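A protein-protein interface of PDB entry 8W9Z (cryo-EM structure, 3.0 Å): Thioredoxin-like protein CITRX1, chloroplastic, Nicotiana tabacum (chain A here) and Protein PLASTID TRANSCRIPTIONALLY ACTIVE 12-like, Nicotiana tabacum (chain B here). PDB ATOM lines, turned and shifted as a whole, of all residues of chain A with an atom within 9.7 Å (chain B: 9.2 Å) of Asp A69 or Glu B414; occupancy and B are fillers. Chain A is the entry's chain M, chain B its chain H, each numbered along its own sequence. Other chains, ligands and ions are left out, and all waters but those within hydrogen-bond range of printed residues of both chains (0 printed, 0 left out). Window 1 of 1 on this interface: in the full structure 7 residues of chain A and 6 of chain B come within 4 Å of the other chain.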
ATOM      1  N   GLY A  63      -0.708  -4.267   8.028  1.00  0.00           N
ATOM      2  CA  GLY A  63      -0.279  -3.622   6.801  1.00  0.00           C
ATOM      3  C   GLY A  63       1.164  -3.919   6.445  1.00  0.00           C
ATOM      4  O   GLY A  63       2.065  -3.737   7.265  1.00  0.00           O
ATOM      5  N   VAL A  66       2.431  -0.253   3.840  1.00  0.00           N
ATOM      6  CA  VAL A  66       2.688   0.898   4.696  1.00  0.00           C
ATOM      7  C   VAL A  66       3.138   0.399   6.060  1.00  0.00           C
ATOM      8  O   VAL A  66       2.789  -0.707   6.492  1.00  0.00           O
ATOM      9  CB  VAL A  66       1.450   1.811   4.816  1.00  0.00           C
ATOM     10  CG1 VAL A  66       0.967   2.235   3.439  1.00  0.00           C
ATOM     11  CG2 VAL A  66       0.343   1.115   5.587  1.00  0.00           C
ATOM     12  N   ARG A  67       3.931   1.218   6.742  1.00  0.00           N
ATOM     13  CA  ARG A  67       4.459   0.885   8.057  1.00  0.00           C
ATOM     14  C   ARG A  67       3.606   1.541   9.135  1.00  0.00           C
ATOM     15  O   ARG A  67       3.105   2.654   8.954  1.00  0.00           O
ATOM     16  CB  ARG A  67       5.915   1.338   8.185  1.00  0.00           C
ATOM     17  CG  ARG A  67       6.602   0.922   9.476  1.00  0.00           C
ATOM     18  CD  ARG A  67       6.749  -0.587   9.565  1.00  0.00           C
ATOM     19  NE  ARG A  67       7.476  -0.994  10.764  1.00  0.00           N
ATOM     20  CZ  ARG A  67       7.726  -2.256  11.093  1.00  0.00           C
ATOM     21  NH1 ARG A  67       7.306  -3.242  10.311  1.00  0.00           N
ATOM     22  NH2 ARG A  67       8.395  -2.534  12.203  1.00  0.00           N
ATOM     23  N   GLU A  68       3.440   0.842  10.254  1.00  0.00           N
ATOM     24  CA  GLU A  68       2.673   1.382  11.368  1.00  0.00           C
ATOM     25  C   GLU A  68       3.374   2.600  11.955  1.00  0.00           C
ATOM     26  O   GLU A  68       4.590   2.593  12.171  1.00  0.00           O
ATOM     27  CB  GLU A  68       2.476   0.318  12.448  1.00  0.00           C
ATOM     28  CG  GLU A  68       1.619  -0.868  12.024  1.00  0.00           C
ATOM     29  CD  GLU A  68       2.377  -1.872  11.174  1.00  0.00           C
ATOM     30  OE1 GLU A  68       3.614  -1.742  11.056  1.00  0.00           O
ATOM     31  OE2 GLU A  68       1.734  -2.791  10.625  1.00  0.00           O
ATOM     32  N   ASP A  69       2.597   3.652  12.213  1.00  0.00           N
ATOM     33  CA  ASP A  69       3.167   4.874  12.769  1.00  0.00           C
ATOM     34  C   ASP A  69       3.615   4.665  14.211  1.00  0.00           C
ATOM     35  O   ASP A  69       4.687   5.129  14.613  1.00  0.00           O
ATOM     36  CB  ASP A  69       2.151   6.014  12.682  1.00  0.00           C
ATOM     37  CG  ASP A  69       1.550   6.155  11.299  1.00  0.00           C
ATOM     38  OD1 ASP A  69       2.203   5.739  10.320  1.00  0.00           O
ATOM     39  OD2 ASP A  69       0.425   6.684  11.192  1.00  0.00           O
ATOM     40  N   TYR A  70       2.804   3.967  15.001  1.00  0.00           N
ATOM     41  CA  TYR A  70       3.082   3.738  16.410  1.00  0.00           C
ATOM     42  C   TYR A  70       3.521   2.296  16.625  1.00  0.00           C
ATOM     43  O   TYR A  70       3.019   1.378  15.971  1.00  0.00           O
ATOM     44  CB  TYR A  70       1.846   4.051  17.254  1.00  0.00           C
ATOM     45  CG  TYR A  70       1.280   5.431  16.999  1.00  0.00           C
ATOM     46  CD1 TYR A  70       0.326   5.642  16.012  1.00  0.00           C
ATOM     47  CD2 TYR A  70       1.704   6.523  17.742  1.00  0.00           C
ATOM     48  CE1 TYR A  70      -0.189   6.902  15.776  1.00  0.00           C
ATOM     49  CE2 TYR A  70       1.195   7.784  17.512  1.00  0.00           C
ATOM     50  CZ  TYR A  70       0.250   7.969  16.529  1.00  0.00           C
ATOM     51  OH  TYR A  70      -0.258   9.227  16.302  1.00  0.00           O
ATOM     52  N   LEU A  71       4.466   2.101  17.548  1.00  0.00           N
ATOM     53  CA  LEU A  71       5.064   0.794  17.777  1.00  0.00           C
ATOM     54  C   LEU A  71       4.772   0.196  19.145  1.00  0.00           C
ATOM     55  O   LEU A  71       4.937  -1.017  19.310  1.00  0.00           O
ATOM     56  CB  LEU A  71       6.590   0.856  17.591  1.00  0.00           C
ATOM     57  CG  LEU A  71       7.150   0.885  16.167  1.00  0.00           C
ATOM     58  CD1 LEU A  71       6.941   2.238  15.501  1.00  0.00           C
ATOM     59  CD2 LEU A  71       8.625   0.511  16.169  1.00  0.00           C
ATOM     60  N   VAL A  72       4.349   0.994  20.120  1.00  0.00           N
ATOM     61  CA  VAL A  72       4.044   0.491  21.455  1.00  0.00           C
ATOM     62  C   VAL A  72       2.589   0.043  21.477  1.00  0.00           C
ATOM     63  O   VAL A  72       1.675   0.861  21.322  1.00  0.00           O
ATOM     64  CB  VAL A  72       4.314   1.556  22.527  1.00  0.00           C
ATOM     65  CG1 VAL A  72       4.009   1.002  23.907  1.00  0.00           C
ATOM     66  CG2 VAL A  72       5.751   2.033  22.447  1.00  0.00           C
ATOM     67  N   LYS A  73       2.373  -1.254  21.674  1.00  0.00           N
ATOM     68  CA  LYS A  73       1.037  -1.829  21.646  1.00  0.00           C
ATOM     69  C   LYS A  73       0.399  -1.783  23.027  1.00  0.00           C
ATOM     70  O   LYS A  73       1.084  -1.786  24.053  1.00  0.00           O
ATOM     71  CB  LYS A  73       1.085  -3.272  21.141  1.00  0.00           C
ATOM     72  CG  LYS A  73       1.693  -3.420  19.758  1.00  0.00           C
ATOM     73  CD  LYS A  73       0.941  -2.583  18.737  1.00  0.00           C
ATOM     74  CE  LYS A  73       1.574  -2.687  17.360  1.00  0.00           C
ATOM     75  NZ  LYS A  73       0.869  -1.836  16.362  1.00  0.00           N
ATOM     76  N   ALA A 108       5.180   9.299  26.110  1.00  0.00           N
ATOM     77  CA  ALA A 108       4.920   8.435  24.963  1.00  0.00           C
ATOM     78  C   ALA A 108       6.007   8.575  23.906  1.00  0.00           C
ATOM     79  O   ALA A 108       6.434   7.580  23.309  1.00  0.00           O
ATOM     80  CB  ALA A 108       3.548   8.754  24.369  1.00  0.00           C
ATOM     81  N   GLU A 112       8.476   5.629  22.627  1.00  0.00           N
ATOM     82  CA  GLU A 112       8.588   5.259  21.219  1.00  0.00           C
ATOM     83  C   GLU A 112      10.034   5.314  20.745  1.00  0.00           C
ATOM     84  O   GLU A 112      10.480   4.436  19.996  1.00  0.00           O
ATOM     85  CB  GLU A 112       7.708   6.166  20.362  1.00  0.00           C
ATOM     86  CG  GLU A 112       6.232   5.847  20.452  1.00  0.00           C
ATOM     87  CD  GLU A 112       5.406   6.651  19.474  1.00  0.00           C
ATOM     88  OE1 GLU A 112       5.696   7.852  19.291  1.00  0.00           O
ATOM     89  OE2 GLU A 112       4.474   6.075  18.878  1.00  0.00           O
ATOM     90  N   MET A 113      10.786   6.333  21.167  1.00  0.00           N
ATOM     91  CA  MET A 113      12.201   6.377  20.818  1.00  0.00           C
ATOM     92  C   MET A 113      12.961   5.199  21.415  1.00  0.00           C
ATOM     93  O   MET A 113      13.831   4.622  20.750  1.00  0.00           O
ATOM     94  CB  MET A 113      12.821   7.696  21.277  1.00  0.00           C
ATOM     95  CG  MET A 113      12.362   8.903  20.478  1.00  0.00           C
ATOM     96  SD  MET A 113      12.789   8.755  18.732  1.00  0.00           S
ATOM     97  CE  MET A 113      14.567   8.581  18.833  1.00  0.00           C
ATOM     98  N   ALA A 115      11.706   2.276  22.059  1.00  0.00           N
ATOM     99  CA  ALA A 115      11.315   1.089  21.309  1.00  0.00           C
ATOM    100  C   ALA A 115      11.983   1.046  19.942  1.00  0.00           C
ATOM    101  O   ALA A 115      12.258  -0.041  19.421  1.00  0.00           O
ATOM    102  CB  ALA A 115       9.795   1.036  21.160  1.00  0.00           C
ATOM    103  N   VAL A 116      12.243   2.210  19.346  1.00  0.00           N
ATOM    104  CA  VAL A 116      12.977   2.248  18.086  1.00  0.00           C
ATOM    105  C   VAL A 116      14.439   1.877  18.306  1.00  0.00           C
ATOM    106  O   VAL A 116      15.050   1.200  17.472  1.00  0.00           O
ATOM    107  CB  VAL A 116      12.827   3.632  17.428  1.00  0.00           C
ATOM    108  CG1 VAL A 116      13.761   3.768  16.237  1.00  0.00           C
ATOM    109  CG2 VAL A 116      11.390   3.853  16.992  1.00  0.00           C
ATOM    110  N   TYR B 407       8.660  16.511  13.984  1.00  0.00           N
ATOM    111  CA  TYR B 407       7.293  16.468  13.484  1.00  0.00           C
ATOM    112  C   TYR B 407       6.445  15.390  14.143  1.00  0.00           C
ATOM    113  O   TYR B 407       5.247  15.306  13.853  1.00  0.00           O
ATOM    114  CB  TYR B 407       7.299  16.279  11.967  1.00  0.00           C
ATOM    115  CG  TYR B 407       7.805  17.493  11.228  1.00  0.00           C
ATOM    116  CD1 TYR B 407       7.075  18.673  11.218  1.00  0.00           C
ATOM    117  CD2 TYR B 407       9.011  17.464  10.546  1.00  0.00           C
ATOM    118  CE1 TYR B 407       7.532  19.788  10.549  1.00  0.00           C
ATOM    119  CE2 TYR B 407       9.473  18.575   9.873  1.00  0.00           C
ATOM    120  CZ  TYR B 407       8.731  19.734   9.878  1.00  0.00           C
ATOM    121  OH  TYR B 407       9.191  20.843   9.207  1.00  0.00           O
ATOM    122  N   ARG B 408       7.028  14.568  15.011  1.00  0.00           N
ATOM    123  CA  ARG B 408       6.258  13.615  15.808  1.00  0.00           C
ATOM    124  C   ARG B 408       5.913  14.227  17.166  1.00  0.00           C
ATOM    125  O   ARG B 408       6.234  13.700  18.230  1.00  0.00           O
ATOM    126  CB  ARG B 408       7.029  12.309  15.960  1.00  0.00           C
ATOM    127  CG  ARG B 408       7.177  11.543  14.662  1.00  0.00           C
ATOM    128  CD  ARG B 408       5.839  11.004  14.192  1.00  0.00           C
ATOM    129  NE  ARG B 408       5.456   9.799  14.918  1.00  0.00           N
ATOM    130  CZ  ARG B 408       4.338   9.118  14.697  1.00  0.00           C
ATOM    131  NH1 ARG B 408       4.071   8.029  15.403  1.00  0.00           N
ATOM    132  NH2 ARG B 408       3.487   9.526  13.766  1.00  0.00           N
ATOM    133  N   GLY B 409       5.243  15.375  17.103  1.00  0.00           N
ATOM    134  CA  GLY B 409       4.885  16.116  18.285  1.00  0.00           C
ATOM    135  C   GLY B 409       3.387  16.258  18.441  1.00  0.00           C
ATOM    136  O   GLY B 409       2.608  15.907  17.551  1.00  0.00           O
ATOM    137  N   PRO B 410       2.954  16.781  19.592  1.00  0.00           N
ATOM    138  CA  PRO B 410       1.512  16.909  19.850  1.00  0.00           C
ATOM    139  C   PRO B 410       0.808  17.921  18.963  1.00  0.00           C
ATOM    140  O   PRO B 410      -0.429  17.927  18.934  1.00  0.00           O
ATOM    141  CB  PRO B 410       1.455  17.339  21.323  1.00  0.00           C
ATOM    142  CG  PRO B 410       2.794  16.980  21.888  1.00  0.00           C
ATOM    143  CD  PRO B 410       3.760  17.148  20.766  1.00  0.00           C
ATOM    144  N   ASP B 411       1.540  18.773  18.243  1.00  0.00           N
ATOM    145  CA  ASP B 411       0.935  19.829  17.442  1.00  0.00           C
ATOM    146  C   ASP B 411       1.138  19.621  15.944  1.00  0.00           C
ATOM    147  O   ASP B 411       1.077  20.586  15.176  1.00  0.00           O
ATOM    148  CB  ASP B 411       1.483  21.192  17.866  1.00  0.00           C
ATOM    149  CG  ASP B 411       2.998  21.227  17.903  1.00  0.00           C
ATOM    150  OD1 ASP B 411       3.624  20.160  17.733  1.00  0.00           O
ATOM    151  OD2 ASP B 411       3.564  22.323  18.101  1.00  0.00           O
ATOM    152  N   PHE B 412       1.372  18.384  15.510  1.00  0.00           N
ATOM    153  CA  PHE B 412       1.545  18.072  14.100  1.00  0.00           C
ATOM    154  C   PHE B 412       0.667  16.887  13.727  1.00  0.00           C
ATOM    155  O   PHE B 412       0.501  15.953  14.514  1.00  0.00           O
ATOM    156  CB  PHE B 412       3.008  17.762  13.767  1.00  0.00           C
ATOM    157  CG  PHE B 412       3.910  18.958  13.834  1.00  0.00           C
ATOM    158  CD1 PHE B 412       3.960  19.863  12.789  1.00  0.00           C
ATOM    159  CD2 PHE B 412       4.716  19.173  14.938  1.00  0.00           C
ATOM    160  CE1 PHE B 412       4.788  20.962  12.846  1.00  0.00           C
ATOM    161  CE2 PHE B 412       5.548  20.272  15.000  1.00  0.00           C
ATOM    162  CZ  PHE B 412       5.584  21.167  13.953  1.00  0.00           C
ATOM    163  N   HIS B 413       0.114  16.934  12.518  1.00  0.00           N
ATOM    164  CA  HIS B 413      -0.768  15.881  12.045  1.00  0.00           C
ATOM    165  C   HIS B 413       0.016  14.594  11.793  1.00  0.00           C
ATOM    166  O   HIS B 413       1.248  14.557  11.840  1.00  0.00           O
ATOM    167  CB  HIS B 413      -1.490  16.321  10.772  1.00  0.00           C
ATOM    168  CG  HIS B 413      -0.570  16.683   9.649  1.00  0.00           C
ATOM    169  ND1 HIS B 413       0.066  15.740   8.872  1.00  0.00           N
ATOM    170  CD2 HIS B 413      -0.180  17.888   9.171  1.00  0.00           C
ATOM    171  CE1 HIS B 413       0.809  16.347   7.964  1.00  0.00           C
ATOM    172  NE2 HIS B 413       0.677  17.651   8.123  1.00  0.00           N
ATOM    173  N   GLU B 414      -0.726  13.523  11.526  1.00  0.00           N
ATOM    174  CA  GLU B 414      -0.112  12.237  11.249  1.00  0.00           C
ATOM    175  C   GLU B 414       0.645  12.285   9.922  1.00  0.00           C
ATOM    176  O   GLU B 414       0.317  13.083   9.040  1.00  0.00           O
ATOM    177  CB  GLU B 414      -1.173  11.141  11.205  1.00  0.00           C
ATOM    178  CG  GLU B 414      -1.959  10.988  12.496  1.00  0.00           C
ATOM    179  CD  GLU B 414      -1.104  10.497  13.647  1.00  0.00           C
ATOM    180  OE1 GLU B 414      -0.074   9.838  13.390  1.00  0.00           O
ATOM    181  OE2 GLU B 414      -1.461  10.770  14.812  1.00  0.00           O
ATOM    182  N   PRO B 415       1.671  11.450   9.762  1.00  0.00           N
ATOM    183  CA  PRO B 415       2.429  11.450   8.504  1.00  0.00           C
ATOM    184  C   PRO B 415       1.550  11.053   7.328  1.00  0.00           C
ATOM    185  O   PRO B 415       0.804  10.074   7.389  1.00  0.00           O
ATOM    186  CB  PRO B 415       3.536  10.420   8.759  1.00  0.00           C
ATOM    187  CG  PRO B 415       3.660  10.354  10.242  1.00  0.00           C
ATOM    188  CD  PRO B 415       2.274  10.559  10.767  1.00  0.00           C
ATOM    189  N   THR B 416       1.646  11.827   6.249  1.00  0.00           N
ATOM    190  CA  THR B 416       0.866  11.565   5.047  1.00  0.00           C
ATOM    191  C   THR B 416       1.496  10.423   4.262  1.00  0.00           C
ATOM    192  O   THR B 416       2.620  10.557   3.763  1.00  0.00           O
ATOM    193  CB  THR B 416       0.770  12.819   4.177  1.00  0.00           C
ATOM    194  OG1 THR B 416       2.086  13.244   3.801  1.00  0.00           O
ATOM    195  CG2 THR B 416       0.076  13.941   4.932  1.00  0.00           C
ATOM    196  N   PRO B 417       0.810   9.291   4.131  1.00  0.00           N
ATOM    197  CA  PRO B 417       1.395   8.157   3.411  1.00  0.00           C
ATOM    198  C   PRO B 417       1.379   8.387   1.909  1.00  0.00           C
ATOM    199  O   PRO B 417       0.653   9.235   1.385  1.00  0.00           O
ATOM    200  CB  PRO B 417       0.486   6.989   3.802  1.00  0.00           C
ATOM    201  CG  PRO B 417      -0.835   7.632   4.048  1.00  0.00           C
ATOM    202  CD  PRO B 417      -0.541   8.991   4.634  1.00  0.00           C
ATOM    203  N   GLU B 425      -2.600  -0.780  -0.169  1.00  0.00           N
ATOM    204  CA  GLU B 425      -2.883  -1.520   1.057  1.00  0.00           C
ATOM    205  C   GLU B 425      -4.373  -1.797   1.205  1.00  0.00           C
ATOM    206  O   GLU B 425      -4.771  -2.907   1.574  1.00  0.00           O
ATOM    207  CB  GLU B 425      -2.365  -0.750   2.270  1.00  0.00           C
ATOM    208  CG  GLU B 425      -2.645  -1.439   3.594  1.00  0.00           C
ATOM    209  CD  GLU B 425      -2.618  -0.480   4.766  1.00  0.00           C
ATOM    210  OE1 GLU B 425      -2.723   0.743   4.537  1.00  0.00           O
ATOM    211  OE2 GLU B 425      -2.491  -0.950   5.918  1.00  0.00           O
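The side-chain hydroxyl (OH) of Tyr A70 sits at hydrogen-bond distance from the side-chain carboxylate (OE2) of Glu B414. The guanidinium group of Arg B408 sits at hydrogen-bond distance from the backbone carbonyl oxygen of Asp A69 (3.1 Å).
NH2 of Arg B408 is in salt-bridge range of OE1 of Glu B414, at 3.6 Å.
CA of Gly A63 touches OE2 of Glu B425, 3.6 Å away. Val A66 touches Glu B425. Glu B414 touches Asp A69. Tyr A70 touches Arg B408 (CE2 to NH1, 3.6 Å).
Printed residues of chain B within 4 Å of Asp A69: Arg B408 and Glu B414. Glu B414 touches just these residues of chain A: Asp A69 and Tyr A70. Of the printed residues of chain B, Tyr A70 touches Arg B408 (3.6 Å) and Glu B414 (2.5 Å). No residue of chain A comes within 4 Å of His B413. Of the printed residues of chain A, Glu B425 touches Gly A63 and Val A66. Printed residues of chain B within 4 Å of Val A66: Glu B425 (3.3 Å). Of the printed residues of chain A, Arg B408 touches Asp A69 and Tyr A70. Of the printed residues of chain B, Gly A63 touches Glu B425. Val A72 touches none of the printed residues of chain B. The nearest residue of chain A that does not touch Glu B414 is Glu A112 (8.1 Å).
Of the 12 printed residues of chain B, 3 touch a printed residue of chain A. Printed residues of chain B that touch a printed residue of chain A: Arg B408, Glu B414 and Glu B425. Of the 14 printed residues of chain A, 4 touch a printed residue of chain B. Printed residues of chain A that touch a printed residue of chain B: Gly A63, Val A66, Asp A69 and Tyr A70. Hydrophobic or aromatic side chains of chain A within 4 Å of the printed part of chain B: Val A66 and Tyr A70. Along chain A the printed residues that touch a printed residue of chain B span positions 63 to 70. Among the printed residues, 6 pairs touch across the chains. Among the printed residues, no Asp or Glu carboxylate lies within 4 Å of a Lys or Arg side-chain nitrogen of the other chain.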
